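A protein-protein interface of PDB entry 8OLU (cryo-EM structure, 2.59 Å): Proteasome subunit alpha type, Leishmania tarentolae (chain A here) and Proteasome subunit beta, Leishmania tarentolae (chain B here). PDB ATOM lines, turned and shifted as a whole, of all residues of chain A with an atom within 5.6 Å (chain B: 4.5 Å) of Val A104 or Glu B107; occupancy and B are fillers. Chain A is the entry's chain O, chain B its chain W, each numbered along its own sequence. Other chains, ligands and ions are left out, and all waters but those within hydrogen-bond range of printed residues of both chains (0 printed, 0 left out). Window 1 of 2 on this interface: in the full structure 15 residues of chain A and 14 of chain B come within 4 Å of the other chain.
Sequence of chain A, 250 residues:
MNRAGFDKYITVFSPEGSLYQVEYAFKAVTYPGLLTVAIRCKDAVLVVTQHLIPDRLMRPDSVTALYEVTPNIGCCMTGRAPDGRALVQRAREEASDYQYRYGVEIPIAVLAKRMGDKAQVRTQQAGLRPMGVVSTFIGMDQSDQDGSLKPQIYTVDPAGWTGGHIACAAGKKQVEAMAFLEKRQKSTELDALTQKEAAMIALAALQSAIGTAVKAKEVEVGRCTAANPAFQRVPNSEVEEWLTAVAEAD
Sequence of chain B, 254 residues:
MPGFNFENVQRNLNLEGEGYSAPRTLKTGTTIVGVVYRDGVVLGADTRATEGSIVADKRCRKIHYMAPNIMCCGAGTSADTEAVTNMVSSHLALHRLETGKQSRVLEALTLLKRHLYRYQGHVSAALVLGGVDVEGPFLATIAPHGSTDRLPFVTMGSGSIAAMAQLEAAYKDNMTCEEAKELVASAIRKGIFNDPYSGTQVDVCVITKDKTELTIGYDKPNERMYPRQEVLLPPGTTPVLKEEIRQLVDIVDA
Of the 10 printed residues of chain A, 6 touch a printed residue of chain B. Printed residues of chain A that touch a printed residue of chain B: Tyr A98, Tyr A100, Arg A101, Tyr A102, Gly A103 and Val A104. Hydrophobic or aromatic side chains of chain A that line the printed part of chain B: Tyr A98, Tyr A102 and Val A104. Of the 11 printed residues of chain B, 5 touch a printed residue of chain A. Hydrophobic or aromatic side chains of chain B that line the printed part of chain A: His B95, Leu B106 and Leu B111. Among the printed residues, no Asp or Glu carboxylate lies within 4 Å of a Lys or Arg side-chain nitrogen of the other chain.
The side-chain carboxylate of Glu B107 is in hydrogen-bond range of the backbone NH of Arg B104 (3.2 Å). O of Leu B106 lies within hydrogen-bond range of OG1 of Thr B110.
The side-chain hydroxyl (OH) of Tyr A98 is in hydrogen-bond range of a ring nitrogen (NE2) of His B95, at 2.8 Å. The backbone carbonyl oxygen (O) of Tyr A102 lies within hydrogen-bond range of the side-chain hydroxyl (OG1) of Thr B110 (3.3 Å).
Among the printed residues, pairs that only touch across the chains: Tyr A102 with Glu B107, Arg A101 with Thr B110, Gly A103 with Thr B110, Tyr A98 with Glu B107, Gly A103 with Leu B106, Val A104 with Glu B107, Tyr A102 with His B95, Arg A101 with Leu B111, Tyr A102 with Leu B106, Tyr A100 with Thr B110, Tyr A102 with Leu B111 and Val A104 with Leu B106.
Printed residues of chain B within 4 Å of Gly A103: Leu B106 and Thr B110. Of chain B, only Leu B106 and Glu B107 come within 4 Å of Val A104. Printed residues of chain A within 4 Å of His B95: Tyr A98 and Tyr A102. Of chain A, only Tyr A98, Tyr A102 and Val A104 come within 4 Å of Glu B107. Of the printed residues of chain A, Thr B110 touches Tyr A100, Arg A101, Tyr A102 and Gly A103. Of the printed residues of chain A, Leu B111 touches Arg A101 and Tyr A102. The nearest printed residue of chain B that does not touch Val A104 is Arg B104 (4.9 Å). The nearest residue of chain A that does not touch Glu B107 is Arg A101 (5.2 Å).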
ATOM      1  N   ALA A  95     -27.437 -28.624  12.833  1.00  0.00           N
ATOM      2  CA  ALA A  95     -28.530 -28.338  11.961  1.00  0.00           C
ATOM      3  C   ALA A  95     -28.375 -26.956  11.369  1.00  0.00           C
ATOM      4  O   ALA A  95     -28.863 -26.723  10.281  1.00  0.00           O
ATOM      5  CB  ALA A  95     -29.801 -28.385  12.797  1.00  0.00           C
ATOM      6  N   TYR A  98     -25.534 -26.762   9.015  1.00  0.00           N
ATOM      7  CA  TYR A  98     -25.907 -27.415   7.795  1.00  0.00           C
ATOM      8  C   TYR A  98     -26.765 -26.526   6.956  1.00  0.00           C
ATOM      9  O   TYR A  98     -26.612 -26.556   5.759  1.00  0.00           O
ATOM     10  CB  TYR A  98     -26.648 -28.718   8.087  1.00  0.00           C
ATOM     11  CG  TYR A  98     -27.093 -29.540   6.917  1.00  0.00           C
ATOM     12  CD1 TYR A  98     -26.401 -30.636   6.490  1.00  0.00           C
ATOM     13  CD2 TYR A  98     -28.184 -29.161   6.171  1.00  0.00           C
ATOM     14  CE1 TYR A  98     -26.871 -31.400   5.444  1.00  0.00           C
ATOM     15  CE2 TYR A  98     -28.587 -29.843   5.054  1.00  0.00           C
ATOM     16  CZ  TYR A  98     -27.973 -31.013   4.726  1.00  0.00           C
ATOM     17  OH  TYR A  98     -28.503 -31.700   3.621  1.00  0.00           O
ATOM     18  N   GLN A  99     -27.677 -25.764   7.542  1.00  0.00           N
ATOM     19  CA  GLN A  99     -28.549 -24.886   6.755  1.00  0.00           C
ATOM     20  C   GLN A  99     -27.713 -23.772   6.113  1.00  0.00           C
ATOM     21  O   GLN A  99     -27.915 -23.374   4.956  1.00  0.00           O
ATOM     22  CB  GLN A  99     -29.683 -24.427   7.659  1.00  0.00           C
ATOM     23  CG  GLN A  99     -30.266 -23.033   7.419  1.00  0.00           C
ATOM     24  CD  GLN A  99     -31.253 -23.042   6.288  1.00  0.00           C
ATOM     25  OE1 GLN A  99     -32.209 -23.816   6.309  1.00  0.00           O
ATOM     26  NE2 GLN A  99     -31.006 -22.173   5.307  1.00  0.00           N
ATOM     27  N   TYR A 100     -26.714 -23.310   6.867  1.00  0.00           N
ATOM     28  CA  TYR A 100     -25.867 -22.293   6.322  1.00  0.00           C
ATOM     29  C   TYR A 100     -25.088 -22.836   5.138  1.00  0.00           C
ATOM     30  O   TYR A 100     -24.975 -22.174   4.135  1.00  0.00           O
ATOM     31  CB  TYR A 100     -25.007 -21.653   7.405  1.00  0.00           C
ATOM     32  CG  TYR A 100     -24.213 -20.479   6.891  1.00  0.00           C
ATOM     33  CD1 TYR A 100     -24.863 -19.313   6.534  1.00  0.00           C
ATOM     34  CD2 TYR A 100     -22.850 -20.570   6.628  1.00  0.00           C
ATOM     35  CE1 TYR A 100     -24.183 -18.247   5.949  1.00  0.00           C
ATOM     36  CE2 TYR A 100     -22.150 -19.508   6.061  1.00  0.00           C
ATOM     37  CZ  TYR A 100     -22.813 -18.328   5.729  1.00  0.00           C
ATOM     38  OH  TYR A 100     -22.194 -17.218   5.175  1.00  0.00           O
ATOM     39  N   ARG A 101     -24.553 -24.030   5.234  1.00  0.00           N
ATOM     40  CA  ARG A 101     -23.689 -24.553   4.212  1.00  0.00           C
ATOM     41  C   ARG A 101     -24.517 -24.945   3.004  1.00  0.00           C
ATOM     42  O   ARG A 101     -24.099 -24.700   1.912  1.00  0.00           O
ATOM     43  CB  ARG A 101     -22.840 -25.677   4.787  1.00  0.00           C
ATOM     44  CG  ARG A 101     -22.022 -26.414   3.746  1.00  0.00           C
ATOM     45  CD  ARG A 101     -21.186 -27.650   4.162  1.00  0.00           C
ATOM     46  NE  ARG A 101     -19.938 -27.345   4.858  1.00  0.00           N
ATOM     47  CZ  ARG A 101     -19.865 -26.783   6.065  1.00  0.00           C
ATOM     48  NH1 ARG A 101     -20.871 -26.871   6.925  1.00  0.00           N
ATOM     49  NH2 ARG A 101     -18.761 -26.145   6.411  1.00  0.00           N
ATOM     50  N   TYR A 102     -25.687 -25.513   3.138  1.00  0.00           N
ATOM     51  CA  TYR A 102     -26.354 -26.064   1.983  1.00  0.00           C
ATOM     52  C   TYR A 102     -27.619 -25.291   1.617  1.00  0.00           C
ATOM     53  O   TYR A 102     -28.340 -25.638   0.719  1.00  0.00           O
ATOM     54  CB  TYR A 102     -26.704 -27.518   2.244  1.00  0.00           C
ATOM     55  CG  TYR A 102     -25.509 -28.398   2.465  1.00  0.00           C
ATOM     56  CD1 TYR A 102     -24.716 -28.821   1.427  1.00  0.00           C
ATOM     57  CD2 TYR A 102     -25.121 -28.791   3.730  1.00  0.00           C
ATOM     58  CE1 TYR A 102     -23.603 -29.620   1.646  1.00  0.00           C
ATOM     59  CE2 TYR A 102     -24.025 -29.602   3.970  1.00  0.00           C
ATOM     60  CZ  TYR A 102     -23.232 -30.002   2.919  1.00  0.00           C
ATOM     61  OH  TYR A 102     -22.109 -30.778   3.149  1.00  0.00           O
ATOM     62  N   GLY A 103     -27.994 -24.315   2.386  1.00  0.00           N
ATOM     63  CA  GLY A 103     -29.184 -23.593   2.043  1.00  0.00           C
ATOM     64  C   GLY A 103     -30.486 -24.339   2.285  1.00  0.00           C
ATOM     65  O   GLY A 103     -31.533 -23.843   1.861  1.00  0.00           O
ATOM     66  N   VAL A 104     -30.437 -25.517   2.901  1.00  0.00           N
ATOM     67  CA  VAL A 104     -31.669 -26.244   3.155  1.00  0.00           C
ATOM     68  C   VAL A 104     -31.653 -26.782   4.565  1.00  0.00           C
ATOM     69  O   VAL A 104     -30.641 -26.867   5.204  1.00  0.00           O
ATOM     70  CB  VAL A 104     -31.931 -27.358   2.135  1.00  0.00           C
ATOM     71  CG1 VAL A 104     -31.865 -26.816   0.727  1.00  0.00           C
ATOM     72  CG2 VAL A 104     -30.948 -28.483   2.251  1.00  0.00           C
ATOM     73  N   GLU A 105     -32.826 -27.039   5.067  1.00  0.00           N
ATOM     74  CA  GLU A 105     -32.973 -27.617   6.376  1.00  0.00           C
ATOM     75  C   GLU A 105     -32.431 -29.049   6.320  1.00  0.00           C
ATOM     76  O   GLU A 105     -32.588 -29.795   5.351  1.00  0.00           O
ATOM     77  CB  GLU A 105     -34.457 -27.508   6.685  1.00  0.00           C
ATOM     78  CG  GLU A 105     -34.743 -27.544   8.160  1.00  0.00           C
ATOM     79  CD  GLU A 105     -35.791 -28.585   8.541  1.00  0.00           C
ATOM     80  OE1 GLU A 105     -35.466 -29.497   9.362  1.00  0.00           O
ATOM     81  OE2 GLU A 105     -36.913 -28.504   7.984  1.00  0.00           O
ATOM     82  N   ILE A 106     -31.752 -29.419   7.383  1.00  0.00           N
ATOM     83  CA  ILE A 106     -31.081 -30.688   7.468  1.00  0.00           C
ATOM     84  C   ILE A 106     -32.112 -31.786   7.552  1.00  0.00           C
ATOM     85  O   ILE A 106     -33.114 -31.693   8.254  1.00  0.00           O
ATOM     86  CB  ILE A 106     -30.130 -30.721   8.656  1.00  0.00           C
ATOM     87  CG1 ILE A 106     -29.311 -31.994   8.645  1.00  0.00           C
ATOM     88  CG2 ILE A 106     -30.823 -30.552  10.003  1.00  0.00           C
ATOM     89  CD1 ILE A 106     -28.133 -31.873   9.543  1.00  0.00           C
ATOM     90  N   LEU B  92     -21.290 -32.500  -3.743  1.00  0.00           N
ATOM     91  CA  LEU B  92     -22.595 -33.049  -3.840  1.00  0.00           C
ATOM     92  C   LEU B  92     -22.611 -34.541  -4.035  1.00  0.00           C
ATOM     93  O   LEU B  92     -23.586 -35.179  -3.650  1.00  0.00           O
ATOM     94  CB  LEU B  92     -23.282 -32.477  -5.049  1.00  0.00           C
ATOM     95  CG  LEU B  92     -23.533 -30.997  -5.061  1.00  0.00           C
ATOM     96  CD1 LEU B  92     -24.095 -30.624  -6.431  1.00  0.00           C
ATOM     97  CD2 LEU B  92     -24.469 -30.575  -3.984  1.00  0.00           C
ATOM     98  N   HIS B  95     -22.281 -35.772  -0.635  1.00  0.00           N
ATOM     99  CA  HIS B  95     -23.400 -35.407   0.188  1.00  0.00           C
ATOM    100  C   HIS B  95     -24.532 -36.345  -0.129  1.00  0.00           C
ATOM    101  O   HIS B  95     -25.364 -36.586   0.698  1.00  0.00           O
ATOM    102  CB  HIS B  95     -23.770 -33.965  -0.101  1.00  0.00           C
ATOM    103  CG  HIS B  95     -24.798 -33.462   0.843  1.00  0.00           C
ATOM    104  ND1 HIS B  95     -24.583 -33.430   2.185  1.00  0.00           N
ATOM    105  CD2 HIS B  95     -26.094 -33.099   0.592  1.00  0.00           C
ATOM    106  CE1 HIS B  95     -25.743 -33.117   2.755  1.00  0.00           C
ATOM    107  NE2 HIS B  95     -26.700 -32.889   1.789  1.00  0.00           N
ATOM    108  N   SER B 103     -29.554 -34.740  -5.196  1.00  0.00           N
ATOM    109  CA  SER B 103     -29.048 -33.440  -4.854  1.00  0.00           C
ATOM    110  C   SER B 103     -30.063 -32.400  -5.230  1.00  0.00           C
ATOM    111  O   SER B 103     -30.691 -32.457  -6.276  1.00  0.00           O
ATOM    112  CB  SER B 103     -27.780 -33.166  -5.532  1.00  0.00           C
ATOM    113  OG  SER B 103     -26.752 -34.078  -5.157  1.00  0.00           O
ATOM    114  N   ARG B 104     -30.203 -31.426  -4.363  1.00  0.00           N
ATOM    115  CA  ARG B 104     -31.101 -30.329  -4.626  1.00  0.00           C
ATOM    116  C   ARG B 104     -30.324 -29.226  -5.351  1.00  0.00           C
ATOM    117  O   ARG B 104     -29.190 -28.886  -5.027  1.00  0.00           O
ATOM    118  CB  ARG B 104     -31.647 -29.694  -3.358  1.00  0.00           C
ATOM    119  CG  ARG B 104     -32.397 -30.594  -2.394  1.00  0.00           C
ATOM    120  CD  ARG B 104     -33.689 -31.124  -2.912  1.00  0.00           C
ATOM    121  NE  ARG B 104     -34.381 -31.887  -1.869  1.00  0.00           N
ATOM    122  CZ  ARG B 104     -35.386 -31.420  -1.131  1.00  0.00           C
ATOM    123  NH1 ARG B 104     -36.216 -32.266  -0.544  1.00  0.00           N
ATOM    124  NH2 ARG B 104     -35.557 -30.108  -1.023  1.00  0.00           N
ATOM    125  N   VAL B 105     -30.982 -28.600  -6.321  1.00  0.00           N
ATOM    126  CA  VAL B 105     -30.295 -27.575  -7.042  1.00  0.00           C
ATOM    127  C   VAL B 105     -29.936 -26.423  -6.129  1.00  0.00           C
ATOM    128  O   VAL B 105     -28.988 -25.694  -6.370  1.00  0.00           O
ATOM    129  CB  VAL B 105     -31.153 -27.088  -8.190  1.00  0.00           C
ATOM    130  CG1 VAL B 105     -30.361 -26.107  -9.033  1.00  0.00           C
ATOM    131  CG2 VAL B 105     -31.671 -28.243  -9.021  1.00  0.00           C
ATOM    132  N   LEU B 106     -30.723 -26.234  -5.095  1.00  0.00           N
ATOM    133  CA  LEU B 106     -30.443 -25.126  -4.228  1.00  0.00           C
ATOM    134  C   LEU B 106     -29.257 -25.423  -3.302  1.00  0.00           C
ATOM    135  O   LEU B 106     -28.600 -24.471  -2.911  1.00  0.00           O
ATOM    136  CB  LEU B 106     -31.731 -24.799  -3.477  1.00  0.00           C
ATOM    137  CG  LEU B 106     -31.550 -23.811  -2.320  1.00  0.00           C
ATOM    138  CD1 LEU B 106     -31.132 -22.389  -2.800  1.00  0.00           C
ATOM    139  CD2 LEU B 106     -32.809 -23.744  -1.515  1.00  0.00           C
ATOM    140  N   GLU B 107     -28.948 -26.705  -2.959  1.00  0.00           N
ATOM    141  CA  GLU B 107     -27.681 -27.024  -2.295  1.00  0.00           C
ATOM    142  C   GLU B 107     -26.541 -26.692  -3.260  1.00  0.00           C
ATOM    143  O   GLU B 107     -25.521 -26.145  -2.896  1.00  0.00           O
ATOM    144  CB  GLU B 107     -27.510 -28.482  -1.825  1.00  0.00           C
ATOM    145  CG  GLU B 107     -28.716 -29.108  -1.092  1.00  0.00           C
ATOM    146  CD  GLU B 107     -28.807 -30.644  -0.844  1.00  0.00           C
ATOM    147  OE1 GLU B 107     -28.415 -31.475  -1.737  1.00  0.00           O
ATOM    148  OE2 GLU B 107     -29.331 -31.047   0.266  1.00  0.00           O
ATOM    149  N   ALA B 108     -26.693 -27.039  -4.515  1.00  0.00           N
ATOM    150  CA  ALA B 108     -25.616 -26.769  -5.450  1.00  0.00           C
ATOM    151  C   ALA B 108     -25.283 -25.284  -5.515  1.00  0.00           C
ATOM    152  O   ALA B 108     -24.146 -24.858  -5.462  1.00  0.00           O
ATOM    153  CB  ALA B 108     -26.022 -27.263  -6.796  1.00  0.00           C
ATOM    154  N   LEU B 109     -26.345 -24.503  -5.589  1.00  0.00           N
ATOM    155  CA  LEU B 109     -26.272 -23.075  -5.653  1.00  0.00           C
ATOM    156  C   LEU B 109     -25.704 -22.525  -4.373  1.00  0.00           C
ATOM    157  O   LEU B 109     -24.927 -21.590  -4.385  1.00  0.00           O
ATOM    158  CB  LEU B 109     -27.679 -22.583  -5.865  1.00  0.00           C
ATOM    159  CG  LEU B 109     -27.817 -21.063  -5.903  1.00  0.00           C
ATOM    160  CD1 LEU B 109     -27.780 -20.588  -7.349  1.00  0.00           C
ATOM    161  CD2 LEU B 109     -29.107 -20.613  -5.294  1.00  0.00           C
ATOM    162  N   THR B 110     -26.091 -23.021  -3.245  1.00  0.00           N
ATOM    163  CA  THR B 110     -25.548 -22.423  -2.052  1.00  0.00           C
ATOM    164  C   THR B 110     -24.060 -22.732  -1.914  1.00  0.00           C
ATOM    165  O   THR B 110     -23.305 -21.906  -1.409  1.00  0.00           O
ATOM    166  CB  THR B 110     -26.203 -22.980  -0.810  1.00  0.00           C
ATOM    167  OG1 THR B 110     -27.589 -22.897  -1.003  1.00  0.00           O
ATOM    168  CG2 THR B 110     -25.857 -22.186   0.408  1.00  0.00           C
ATOM    169  N   LEU B 111     -23.631 -23.929  -2.278  1.00  0.00           N
ATOM    170  CA  LEU B 111     -22.232 -24.226  -2.161  1.00  0.00           C
ATOM    171  C   LEU B 111     -21.402 -23.350  -3.073  1.00  0.00           C
ATOM    172  O   LEU B 111     -20.316 -22.950  -2.738  1.00  0.00           O
ATOM    173  CB  LEU B 111     -22.023 -25.670  -2.577  1.00  0.00           C
ATOM    174  CG  LEU B 111     -22.587 -26.721  -1.612  1.00  0.00           C
ATOM    175  CD1 LEU B 111     -22.493 -28.062  -2.317  1.00  0.00           C
ATOM    176  CD2 LEU B 111     -21.825 -26.804  -0.302  1.00  0.00           C
